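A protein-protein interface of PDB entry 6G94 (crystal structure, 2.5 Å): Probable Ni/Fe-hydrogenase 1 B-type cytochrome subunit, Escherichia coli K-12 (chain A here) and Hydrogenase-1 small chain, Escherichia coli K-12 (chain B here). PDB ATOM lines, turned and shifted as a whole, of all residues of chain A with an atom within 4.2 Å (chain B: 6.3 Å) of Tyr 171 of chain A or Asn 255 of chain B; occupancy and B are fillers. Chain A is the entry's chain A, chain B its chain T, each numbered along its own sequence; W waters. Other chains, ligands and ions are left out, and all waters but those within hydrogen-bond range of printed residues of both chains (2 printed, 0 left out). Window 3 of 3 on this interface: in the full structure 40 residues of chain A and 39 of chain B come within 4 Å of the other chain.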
ATOM      1  N   VAL A 167     -24.091 -12.704  34.698  1.00  0.00           N
ATOM      2  CA  VAL A 167     -24.683 -14.000  34.603  1.00  0.00           C
ATOM      3  C   VAL A 167     -25.752 -13.984  33.521  1.00  0.00           C
ATOM      4  O   VAL A 167     -25.746 -14.820  32.645  1.00  0.00           O
ATOM      5  CB  VAL A 167     -25.212 -14.408  35.978  1.00  0.00           C
ATOM      6  CG1 VAL A 167     -26.176 -15.581  35.887  1.00  0.00           C
ATOM      7  CG2 VAL A 167     -24.043 -14.748  36.874  1.00  0.00           C
ATOM      8  N   GLU A 168     -26.648 -13.007  33.574  1.00  0.00           N
ATOM      9  CA  GLU A 168     -27.729 -12.892  32.598  1.00  0.00           C
ATOM     10  C   GLU A 168     -27.180 -12.693  31.206  1.00  0.00           C
ATOM     11  O   GLU A 168     -27.757 -13.177  30.240  1.00  0.00           O
ATOM     12  CB  GLU A 168     -28.694 -11.768  32.966  1.00  0.00           C
ATOM     13  CG  GLU A 168     -29.059 -11.731  34.437  1.00  0.00           C
ATOM     14  CD  GLU A 168     -30.018 -10.614  34.800  1.00  0.00           C
ATOM     15  OE1 GLU A 168     -30.478  -9.920  33.885  1.00  0.00           O
ATOM     16  OE2 GLU A 168     -30.327 -10.417  35.992  1.00  0.00           O
ATOM     17  N   PHE A 169     -26.058 -11.986  31.119  1.00  0.00           N
ATOM     18  CA  PHE A 169     -25.382 -11.768  29.868  1.00  0.00           C
ATOM     19  C   PHE A 169     -24.926 -13.085  29.243  1.00  0.00           C
ATOM     20  O   PHE A 169     -25.219 -13.366  28.103  1.00  0.00           O
ATOM     21  CB  PHE A 169     -24.198 -10.820  30.048  1.00  0.00           C
ATOM     22  CG  PHE A 169     -23.289 -10.784  28.866  1.00  0.00           C
ATOM     23  CD1 PHE A 169     -23.632 -10.071  27.735  1.00  0.00           C
ATOM     24  CD2 PHE A 169     -22.139 -11.528  28.868  1.00  0.00           C
ATOM     25  CE1 PHE A 169     -22.834 -10.076  26.636  1.00  0.00           C
ATOM     26  CE2 PHE A 169     -21.324 -11.535  27.770  1.00  0.00           C
ATOM     27  CZ  PHE A 169     -21.673 -10.803  26.655  1.00  0.00           C
ATOM     28  N   PHE A 170     -24.201 -13.886  29.997  1.00  0.00           N
ATOM     29  CA  PHE A 170     -23.798 -15.188  29.522  1.00  0.00           C
ATOM     30  C   PHE A 170     -24.974 -16.093  29.165  1.00  0.00           C
ATOM     31  O   PHE A 170     -24.858 -16.922  28.286  1.00  0.00           O
ATOM     32  CB  PHE A 170     -22.840 -15.827  30.500  1.00  0.00           C
ATOM     33  CG  PHE A 170     -21.458 -15.302  30.371  1.00  0.00           C
ATOM     34  CD1 PHE A 170     -20.707 -15.597  29.260  1.00  0.00           C
ATOM     35  CD2 PHE A 170     -20.915 -14.467  31.324  1.00  0.00           C
ATOM     36  CE1 PHE A 170     -19.421 -15.082  29.111  1.00  0.00           C
ATOM     37  CE2 PHE A 170     -19.631 -13.957  31.182  1.00  0.00           C
ATOM     38  CZ  PHE A 170     -18.879 -14.265  30.075  1.00  0.00           C
ATOM     39  N   TYR A 171     -26.106 -15.914  29.830  1.00  0.00           N
ATOM     40  CA  TYR A 171     -27.347 -16.622  29.468  1.00  0.00           C
ATOM     41  C   TYR A 171     -27.900 -16.076  28.160  1.00  0.00           C
ATOM     42  O   TYR A 171     -28.435 -16.818  27.346  1.00  0.00           O
ATOM     43  CB  TYR A 171     -28.421 -16.533  30.584  1.00  0.00           C
ATOM     44  CG  TYR A 171     -28.339 -17.625  31.637  1.00  0.00           C
ATOM     45  CD1 TYR A 171     -27.492 -17.505  32.745  1.00  0.00           C
ATOM     46  CD2 TYR A 171     -29.093 -18.784  31.515  1.00  0.00           C
ATOM     47  CE1 TYR A 171     -27.403 -18.510  33.700  1.00  0.00           C
ATOM     48  CE2 TYR A 171     -29.019 -19.798  32.463  1.00  0.00           C
ATOM     49  CZ  TYR A 171     -28.175 -19.657  33.551  1.00  0.00           C
ATOM     50  OH  TYR A 171     -28.102 -20.655  34.493  1.00  0.00           O
ATOM     51  N   TRP A 172     -27.759 -14.768  27.974  1.00  0.00           N
ATOM     52  CA  TRP A 172     -28.231 -14.085  26.774  1.00  0.00           C
ATOM     53  C   TRP A 172     -27.407 -14.543  25.563  1.00  0.00           C
ATOM     54  O   TRP A 172     -27.942 -14.760  24.493  1.00  0.00           O
ATOM     55  CB  TRP A 172     -28.173 -12.569  26.983  1.00  0.00           C
ATOM     56  CG  TRP A 172     -28.630 -11.759  25.813  1.00  0.00           C
ATOM     57  CD1 TRP A 172     -29.925 -11.495  25.452  1.00  0.00           C
ATOM     58  CD2 TRP A 172     -27.797 -11.085  24.850  1.00  0.00           C
ATOM     59  NE1 TRP A 172     -29.950 -10.709  24.319  1.00  0.00           N
ATOM     60  CE2 TRP A 172     -28.661 -10.444  23.924  1.00  0.00           C
ATOM     61  CE3 TRP A 172     -26.403 -10.970  24.668  1.00  0.00           C
ATOM     62  CZ2 TRP A 172     -28.182  -9.701  22.829  1.00  0.00           C
ATOM     63  CZ3 TRP A 172     -25.926 -10.234  23.577  1.00  0.00           C
ATOM     64  CH2 TRP A 172     -26.817  -9.612  22.671  1.00  0.00           C
ATOM     65  N   THR A 173     -26.102 -14.692  25.768  1.00  0.00           N
ATOM     66  CA  THR A 173     -25.175 -15.396  24.877  1.00  0.00           C
ATOM     67  C   THR A 173     -25.687 -16.762  24.394  1.00  0.00           C
ATOM     68  O   THR A 173     -25.268 -17.264  23.344  1.00  0.00           O
ATOM     69  CB  THR A 173     -23.830 -15.545  25.627  1.00  0.00           C
ATOM     70  OG1 THR A 173     -23.077 -14.355  25.413  1.00  0.00           O
ATOM     71  CG2 THR A 173     -22.999 -16.782  25.242  1.00  0.00           C
ATOM     72  N   GLY A 174     -26.619 -17.340  25.146  1.00  0.00           N
ATOM     73  CA  GLY A 174     -27.068 -18.686  24.881  1.00  0.00           C
ATOM     74  C   GLY A 174     -26.223 -19.666  25.665  1.00  0.00           C
ATOM     75  O   GLY A 174     -26.033 -20.806  25.249  1.00  0.00           O
ATOM     76  N   GLY A 175     -25.721 -19.223  26.817  1.00  0.00           N
ATOM     77  CA  GLY A 175     -24.920 -20.078  27.685  1.00  0.00           C
ATOM     78  C   GLY A 175     -25.384 -20.115  29.117  1.00  0.00           C
ATOM     79  O   GLY A 175     -26.503 -19.712  29.430  1.00  0.00           O
ATOM     80  N   ASN A 176     -24.522 -20.623  29.989  1.00  0.00           N
ATOM     81  CA  ASN A 176     -24.789 -20.647  31.420  1.00  0.00           C
ATOM     82  C   ASN A 176     -23.519 -20.287  32.186  1.00  0.00           C
ATOM     83  O   ASN A 176     -22.491 -19.984  31.584  1.00  0.00           O
ATOM     84  CB  ASN A 176     -25.372 -22.002  31.860  1.00  0.00           C
ATOM     85  CG  ASN A 176     -24.469 -23.186  31.528  1.00  0.00           C
ATOM     86  OD1 ASN A 176     -23.616 -23.578  32.336  1.00  0.00           O
ATOM     87  ND2 ASN A 176     -24.674 -23.784  30.346  1.00  0.00           N
ATOM     88  N   THR B 114     -35.808 -28.623  29.058  1.00  0.00           N
ATOM     89  CA  THR B 114     -34.791 -27.841  28.378  1.00  0.00           C
ATOM     90  C   THR B 114     -35.207 -27.502  26.933  1.00  0.00           C
ATOM     91  O   THR B 114     -34.899 -26.413  26.443  1.00  0.00           O
ATOM     92  CB  THR B 114     -33.425 -28.581  28.423  1.00  0.00           C
ATOM     93  OG1 THR B 114     -33.037 -28.800  29.790  1.00  0.00           O
ATOM     94  CG2 THR B 114     -32.318 -27.786  27.715  1.00  0.00           C
ATOM     95  N   SER B 117     -37.655 -24.555  27.106  1.00  0.00           N
ATOM     96  CA  SER B 117     -36.952 -23.481  27.836  1.00  0.00           C
ATOM     97  C   SER B 117     -35.778 -22.881  27.051  1.00  0.00           C
ATOM     98  O   SER B 117     -35.641 -21.658  26.967  1.00  0.00           O
ATOM     99  CB  SER B 117     -36.430 -23.985  29.195  1.00  0.00           C
ATOM    100  OG  SER B 117     -37.479 -24.438  30.032  1.00  0.00           O
ATOM    101  N   TRP B 118     -34.945 -23.752  26.479  1.00  0.00           N
ATOM    102  CA  TRP B 118     -33.667 -23.348  25.921  1.00  0.00           C
ATOM    103  C   TRP B 118     -33.464 -23.824  24.496  1.00  0.00           C
ATOM    104  O   TRP B 118     -32.999 -23.062  23.665  1.00  0.00           O
ATOM    105  CB  TRP B 118     -32.522 -23.876  26.789  1.00  0.00           C
ATOM    106  CG  TRP B 118     -32.546 -23.437  28.237  1.00  0.00           C
ATOM    107  CD1 TRP B 118     -32.514 -24.246  29.345  1.00  0.00           C
ATOM    108  CD2 TRP B 118     -32.580 -22.089  28.727  1.00  0.00           C
ATOM    109  NE1 TRP B 118     -32.528 -23.485  30.489  1.00  0.00           N
ATOM    110  CE2 TRP B 118     -32.562 -22.158  30.139  1.00  0.00           C
ATOM    111  CE3 TRP B 118     -32.612 -20.825  28.109  1.00  0.00           C
ATOM    112  CZ2 TRP B 118     -32.587 -21.003  30.945  1.00  0.00           C
ATOM    113  CZ3 TRP B 118     -32.636 -19.682  28.915  1.00  0.00           C
ATOM    114  CH2 TRP B 118     -32.623 -19.782  30.314  1.00  0.00           C
ATOM    115  N   GLY B 119     -33.807 -25.076  24.209  1.00  0.00           N
ATOM    116  CA  GLY B 119     -33.600 -25.645  22.878  1.00  0.00           C
ATOM    117  C   GLY B 119     -33.205 -27.109  22.923  1.00  0.00           C
ATOM    118  O   GLY B 119     -33.583 -27.885  22.049  1.00  0.00           O
ATOM    119  N   PRO B 133     -36.245 -21.978  21.294  1.00  0.00           N
ATOM    120  CA  PRO B 133     -37.047 -22.033  22.511  1.00  0.00           C
ATOM    121  C   PRO B 133     -38.269 -21.130  22.380  1.00  0.00           C
ATOM    122  O   PRO B 133     -38.256 -20.178  21.586  1.00  0.00           O
ATOM    123  CB  PRO B 133     -36.087 -21.522  23.589  1.00  0.00           C
ATOM    124  CG  PRO B 133     -35.057 -20.717  22.852  1.00  0.00           C
ATOM    125  CD  PRO B 133     -34.911 -21.387  21.527  1.00  0.00           C
ATOM    126  N   MET B 175     -34.296 -15.582  34.828  1.00  0.00           N
ATOM    127  CA  MET B 175     -34.346 -16.447  33.656  1.00  0.00           C
ATOM    128  C   MET B 175     -35.721 -17.085  33.461  1.00  0.00           C
ATOM    129  O   MET B 175     -35.925 -17.854  32.524  1.00  0.00           O
ATOM    130  CB  MET B 175     -33.291 -17.546  33.784  1.00  0.00           C
ATOM    131  CG  MET B 175     -31.991 -17.258  33.040  1.00  0.00           C
ATOM    132  SD  MET B 175     -31.081 -15.791  33.574  1.00  0.00           S
ATOM    133  CE  MET B 175     -30.536 -16.264  35.219  1.00  0.00           C
ATOM    134  N   ARG B 177     -37.179 -19.202  35.651  1.00  0.00           N
ATOM    135  CA  ARG B 177     -37.259 -20.475  36.360  1.00  0.00           C
ATOM    136  C   ARG B 177     -37.800 -20.263  37.777  1.00  0.00           C
ATOM    137  O   ARG B 177     -37.419 -19.289  38.440  1.00  0.00           O
ATOM    138  CB  ARG B 177     -35.896 -21.146  36.431  1.00  0.00           C
ATOM    139  CG  ARG B 177     -35.206 -21.305  35.100  1.00  0.00           C
ATOM    140  CD  ARG B 177     -33.816 -21.878  35.288  1.00  0.00           C
ATOM    141  NE  ARG B 177     -32.906 -20.917  35.898  1.00  0.00           N
ATOM    142  CZ  ARG B 177     -31.580 -21.031  35.895  1.00  0.00           C
ATOM    143  NH1 ARG B 177     -30.985 -22.066  35.310  1.00  0.00           N
ATOM    144  NH2 ARG B 177     -30.837 -20.099  36.466  1.00  0.00           N
ATOM    145  N   THR B 225     -22.302 -25.565  38.125  1.00  0.00           N
ATOM    146  CA  THR B 225     -22.849 -24.502  37.293  1.00  0.00           C
ATOM    147  C   THR B 225     -24.289 -24.769  36.878  1.00  0.00           C
ATOM    148  O   THR B 225     -24.813 -24.071  36.010  1.00  0.00           O
ATOM    149  CB  THR B 225     -21.998 -24.305  36.028  1.00  0.00           C
ATOM    150  OG1 THR B 225     -21.827 -25.567  35.362  1.00  0.00           O
ATOM    151  CG2 THR B 225     -20.649 -23.738  36.402  1.00  0.00           C
ATOM    152  N   TYR B 227     -28.344 -25.210  37.889  1.00  0.00           N
ATOM    153  CA  TYR B 227     -29.429 -24.953  38.826  1.00  0.00           C
ATOM    154  C   TYR B 227     -30.540 -25.952  38.657  1.00  0.00           C
ATOM    155  O   TYR B 227     -31.165 -26.010  37.595  1.00  0.00           O
ATOM    156  CB  TYR B 227     -29.999 -23.550  38.615  1.00  0.00           C
ATOM    157  CG  TYR B 227     -29.062 -22.427  39.043  1.00  0.00           C
ATOM    158  CD1 TYR B 227     -28.062 -21.955  38.184  1.00  0.00           C
ATOM    159  CD2 TYR B 227     -29.173 -21.841  40.304  1.00  0.00           C
ATOM    160  CE1 TYR B 227     -27.203 -20.934  38.566  1.00  0.00           C
ATOM    161  CE2 TYR B 227     -28.314 -20.810  40.691  1.00  0.00           C
ATOM    162  CZ  TYR B 227     -27.330 -20.358  39.816  1.00  0.00           C
ATOM    163  OH  TYR B 227     -26.454 -19.341  40.176  1.00  0.00           O
ATOM    164  N   GLY B 251     -25.248 -31.175  33.368  1.00  0.00           N
ATOM    165  CA  GLY B 251     -25.705 -29.787  33.238  1.00  0.00           C
ATOM    166  C   GLY B 251     -27.040 -29.659  32.503  1.00  0.00           C
ATOM    167  O   GLY B 251     -27.392 -28.571  32.042  1.00  0.00           O
ATOM    168  N   CYS B 252     -27.801 -30.757  32.437  1.00  0.00           N
ATOM    169  CA  CYS B 252     -28.973 -30.868  31.559  1.00  0.00           C
ATOM    170  C   CYS B 252     -30.087 -29.838  31.787  1.00  0.00           C
ATOM    171  O   CYS B 252     -30.964 -29.671  30.933  1.00  0.00           O
ATOM    172  CB  CYS B 252     -29.547 -32.295  31.618  1.00  0.00           C
ATOM    173  SG  CYS B 252     -30.740 -32.589  32.949  1.00  0.00           S
ATOM    174  N   ALA B 253     -30.060 -29.165  32.932  1.00  0.00           N
ATOM    175  CA  ALA B 253     -31.054 -28.125  33.240  1.00  0.00           C
ATOM    176  C   ALA B 253     -30.631 -26.755  32.692  1.00  0.00           C
ATOM    177  O   ALA B 253     -31.390 -25.764  32.773  1.00  0.00           O
ATOM    178  CB  ALA B 253     -31.315 -28.048  34.745  1.00  0.00           C
ATOM    179  N   GLU B 254     -29.420 -26.706  32.142  1.00  0.00           N
ATOM    180  CA  GLU B 254     -28.831 -25.426  31.740  1.00  0.00           C
ATOM    181  C   GLU B 254     -28.855 -25.178  30.230  1.00  0.00           C
ATOM    182  O   GLU B 254     -28.677 -26.101  29.420  1.00  0.00           O
ATOM    183  CB  GLU B 254     -27.410 -25.266  32.315  1.00  0.00           C
ATOM    184  CG  GLU B 254     -27.377 -25.118  33.827  1.00  0.00           C
ATOM    185  CD  GLU B 254     -28.121 -23.882  34.297  1.00  0.00           C
ATOM    186  OE1 GLU B 254     -28.604 -23.880  35.456  1.00  0.00           O
ATOM    187  OE2 GLU B 254     -28.224 -22.905  33.519  1.00  0.00           O
ATOM    188  N   ASN B 255     -29.108 -23.920  29.889  1.00  0.00           N
ATOM    189  CA  ASN B 255     -29.107 -23.447  28.527  1.00  0.00           C
ATOM    190  C   ASN B 255     -27.832 -23.795  27.753  1.00  0.00           C
ATOM    191  O   ASN B 255     -26.723 -23.383  28.128  1.00  0.00           O
ATOM    192  CB  ASN B 255     -29.292 -21.939  28.541  1.00  0.00           C
ATOM    193  CG  ASN B 255     -29.480 -21.371  27.159  1.00  0.00           C
ATOM    194  OD1 ASN B 255     -29.985 -22.054  26.254  1.00  0.00           O
ATOM    195  ND2 ASN B 255     -29.083 -20.105  26.983  1.00  0.00           N
ATOM    196  N   GLY B 256     -28.009 -24.548  26.670  1.00  0.00           N
ATOM    197  CA  GLY B 256     -26.925 -24.879  25.758  1.00  0.00           C
ATOM    198  C   GLY B 256     -25.887 -25.831  26.303  1.00  0.00           C
ATOM    199  O   GLY B 256     -24.750 -25.817  25.846  1.00  0.00           O
ATOM    200  N   PHE B 257     -26.267 -26.653  27.260  1.00  0.00           N
ATOM    201  CA  PHE B 257     -25.337 -27.541  27.939  1.00  0.00           C
ATOM    202  C   PHE B 257     -24.688 -28.569  27.036  1.00  0.00           C
ATOM    203  O   PHE B 257     -23.608 -29.048  27.335  1.00  0.00           O
ATOM    204  CB  PHE B 257     -25.997 -28.222  29.164  1.00  0.00           C
ATOM    205  CG  PHE B 257     -26.901 -29.390  28.827  1.00  0.00           C
ATOM    206  CD1 PHE B 257     -28.207 -29.178  28.432  1.00  0.00           C
ATOM    207  CD2 PHE B 257     -26.427 -30.700  28.900  1.00  0.00           C
ATOM    208  CE1 PHE B 257     -29.017 -30.242  28.092  1.00  0.00           C
ATOM    209  CE2 PHE B 257     -27.233 -31.763  28.562  1.00  0.00           C
ATOM    210  CZ  PHE B 257     -28.529 -31.528  28.173  1.00  0.00           C
ATOM    211  N   TRP B 258     -25.371 -28.904  25.944  1.00  0.00           N
ATOM    212  CA  TRP B 258     -24.901 -29.891  24.970  1.00  0.00           C
ATOM    213  C   TRP B 258     -23.571 -29.461  24.354  1.00  0.00           C
ATOM    214  O   TRP B 258     -22.651 -30.270  24.220  1.00  0.00           O
ATOM    215  CB  TRP B 258     -25.936 -30.120  23.862  1.00  0.00           C
ATOM    216  CG  TRP B 258     -27.164 -30.807  24.315  1.00  0.00           C
ATOM    217  CD1 TRP B 258     -28.397 -30.252  24.479  1.00  0.00           C
ATOM    218  CD2 TRP B 258     -27.305 -32.182  24.674  1.00  0.00           C
ATOM    219  NE1 TRP B 258     -29.299 -31.192  24.921  1.00  0.00           N
ATOM    220  CE2 TRP B 258     -28.647 -32.383  25.049  1.00  0.00           C
ATOM    221  CE3 TRP B 258     -26.430 -33.256  24.732  1.00  0.00           C
ATOM    222  CZ2 TRP B 258     -29.114 -33.597  25.472  1.00  0.00           C
ATOM    223  CZ3 TRP B 258     -26.909 -34.463  25.142  1.00  0.00           C
ATOM    224  CH2 TRP B 258     -28.231 -34.626  25.513  1.00  0.00           C
ATOM    225  N   ARG B 260     -21.328 -27.432  25.603  1.00  0.00           N
ATOM    226  CA  ARG B 260     -20.333 -27.070  26.584  1.00  0.00           C
ATOM    227  C   ARG B 260     -19.415 -28.255  26.775  1.00  0.00           C
ATOM    228  O   ARG B 260     -19.312 -28.815  27.877  1.00  0.00           O
ATOM    229  CB  ARG B 260     -20.944 -26.613  27.914  1.00  0.00           C
ATOM    230  CG  ARG B 260     -21.882 -25.417  27.830  1.00  0.00           C
ATOM    231  CD  ARG B 260     -21.280 -24.234  27.107  1.00  0.00           C
ATOM    232  NE  ARG B 260     -22.219 -23.121  26.904  1.00  0.00           N
ATOM    233  CZ  ARG B 260     -22.853 -22.840  25.756  1.00  0.00           C
ATOM    234  NH1 ARG B 260     -22.696 -23.588  24.676  1.00  0.00           N
ATOM    235  NH2 ARG B 260     -23.658 -21.798  25.672  1.00  0.00           N
HETATM  236  O   HOH W   1     -25.773 -21.832  35.127  1.00  0.00           O
HETATM  237  O   HOH W   2     -28.325 -21.641  23.660  1.00  0.00           O
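The backbone carbonyl oxygen (O) of Ala 253 of chain B is in hydrogen-bond range of the indole nitrogen (NE1) of Trp 118 of chain B, at 3.4 Å.
The guanidinium group of Arg 177 of chain B lies within salt-bridge range of the side-chain carboxylate of Glu 254 of chain B.
N of Tyr 227 of chain B sits at hydrogen-bond distance from OE1 of Glu 254 of chain B.
The backbone carbonyl oxygen (O) of Gly 256 of chain B sits at hydrogen-bond distance from the guanidinium group (NH1) of Arg 260 of chain B (3.2 Å).
The backbone NH (N) of Gly 175 of chain A sits at hydrogen-bond distance from the backbone carbonyl oxygen (O) of Phe 170 of chain A, at 2.9 Å.
OH of Tyr 171 of chain A sits at hydrogen-bond distance from NH1 of Arg 177 of chain B (3.3 Å).
The side-chain carboxylate (OE2) of Glu 254 of chain B lies within hydrogen-bond range of the side-chain hydroxyl (OH) of Tyr 171 of chain A, 2.5 Å away.
The side-chain amide nitrogen (ND2) of Asn 255 of chain B sits at hydrogen-bond distance from the backbone carbonyl oxygen (O) of Tyr 171 of chain A (3.4 Å).
ND2 of Asn 255 of chain B lies close to N of Gly 175 of chain A (3.5 Å).
The side-chain amide nitrogen (ND2) of Asn 176 of chain A is in hydrogen-bond range of the backbone carbonyl oxygen (O) of Asn 255 of chain B (3.0 Å).
The guanidinium group (NH2) of Arg 260 of chain B is in hydrogen-bond range of the backbone carbonyl oxygen (O) of Gly 174 of chain A (2.6 Å).
N of Gly 175 of chain A lies close to NH2 of Arg 260 of chain B.
Water W1 lies within hydrogen-bond range of the backbone carbonyl oxygen (O) of Thr 225 of chain B (2.6 Å), the side-chain hydroxyl (OH) of Tyr 171 of chain A (2.7 Å) and the side-chain carboxylate (OE2) of Glu 254 of chain B (3.1 Å).
Water W2 bridges the backbone carbonyl oxygen of Gly 174 of chain A (2.9 Å) and the side-chain amide oxygen of Asn 255 of chain B (3.1 Å).
CH2 of Trp 118 of chain B touches CD2 of Tyr 171 of chain A (3.9 Å).
CD2 of Tyr 171 of chain A touches CG of Met 175 of chain B (3.6 Å).
OH of Tyr 171 of chain A touches CD1 of Tyr 227 of chain B (3.9 Å).
Gly 174 of chain A touches Asn 255 of chain B.
Asn 176 of chain A touches Thr 225 of chain B (OD1 to O, 3.9 Å).
CB of Asn 176 of chain A touches OE2 of Glu 254 of chain B, 3.4 Å away.
Val 167 of chain A touches none of the printed residues of chain B.
Tyr 171 of chain A touches just these residues of chain B: Trp 118 (3.9 Å), Met 175 (3.6 Å), Arg 177 (3.3 Å), Tyr 227 (3.9 Å), Glu 254 (2.5 Å) and Asn 255 (3.4 Å).
Printed residues of chain B within 4 Å of Gly 175 of chain A: Asn 255 (3.5 Å) and Arg 260 (2.9 Å).
Printed residues of chain A within 4 Å of Thr 225 of chain B: Asn 176 (3.9 Å).
Cys 252 of chain B touches none of the printed residues of chain A.
Asn 255 of chain B touches just these residues of chain A: Tyr 171, Gly 174, Gly 175 and Asn 176.
The nearest residue of chain B that does not touch Tyr 171 of chain A is Thr 225 of chain B (5.0 Å).
The nearest printed residue of chain A that does not touch Arg 177 of chain B is Val 167 of chain A (6.5 Å).
Hydrophobic or aromatic side chains of chain B that line the printed part of chain A: Trp 118, Met 175 and Tyr 227.
Among the printed residues, 13 pairs touch across the chains.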
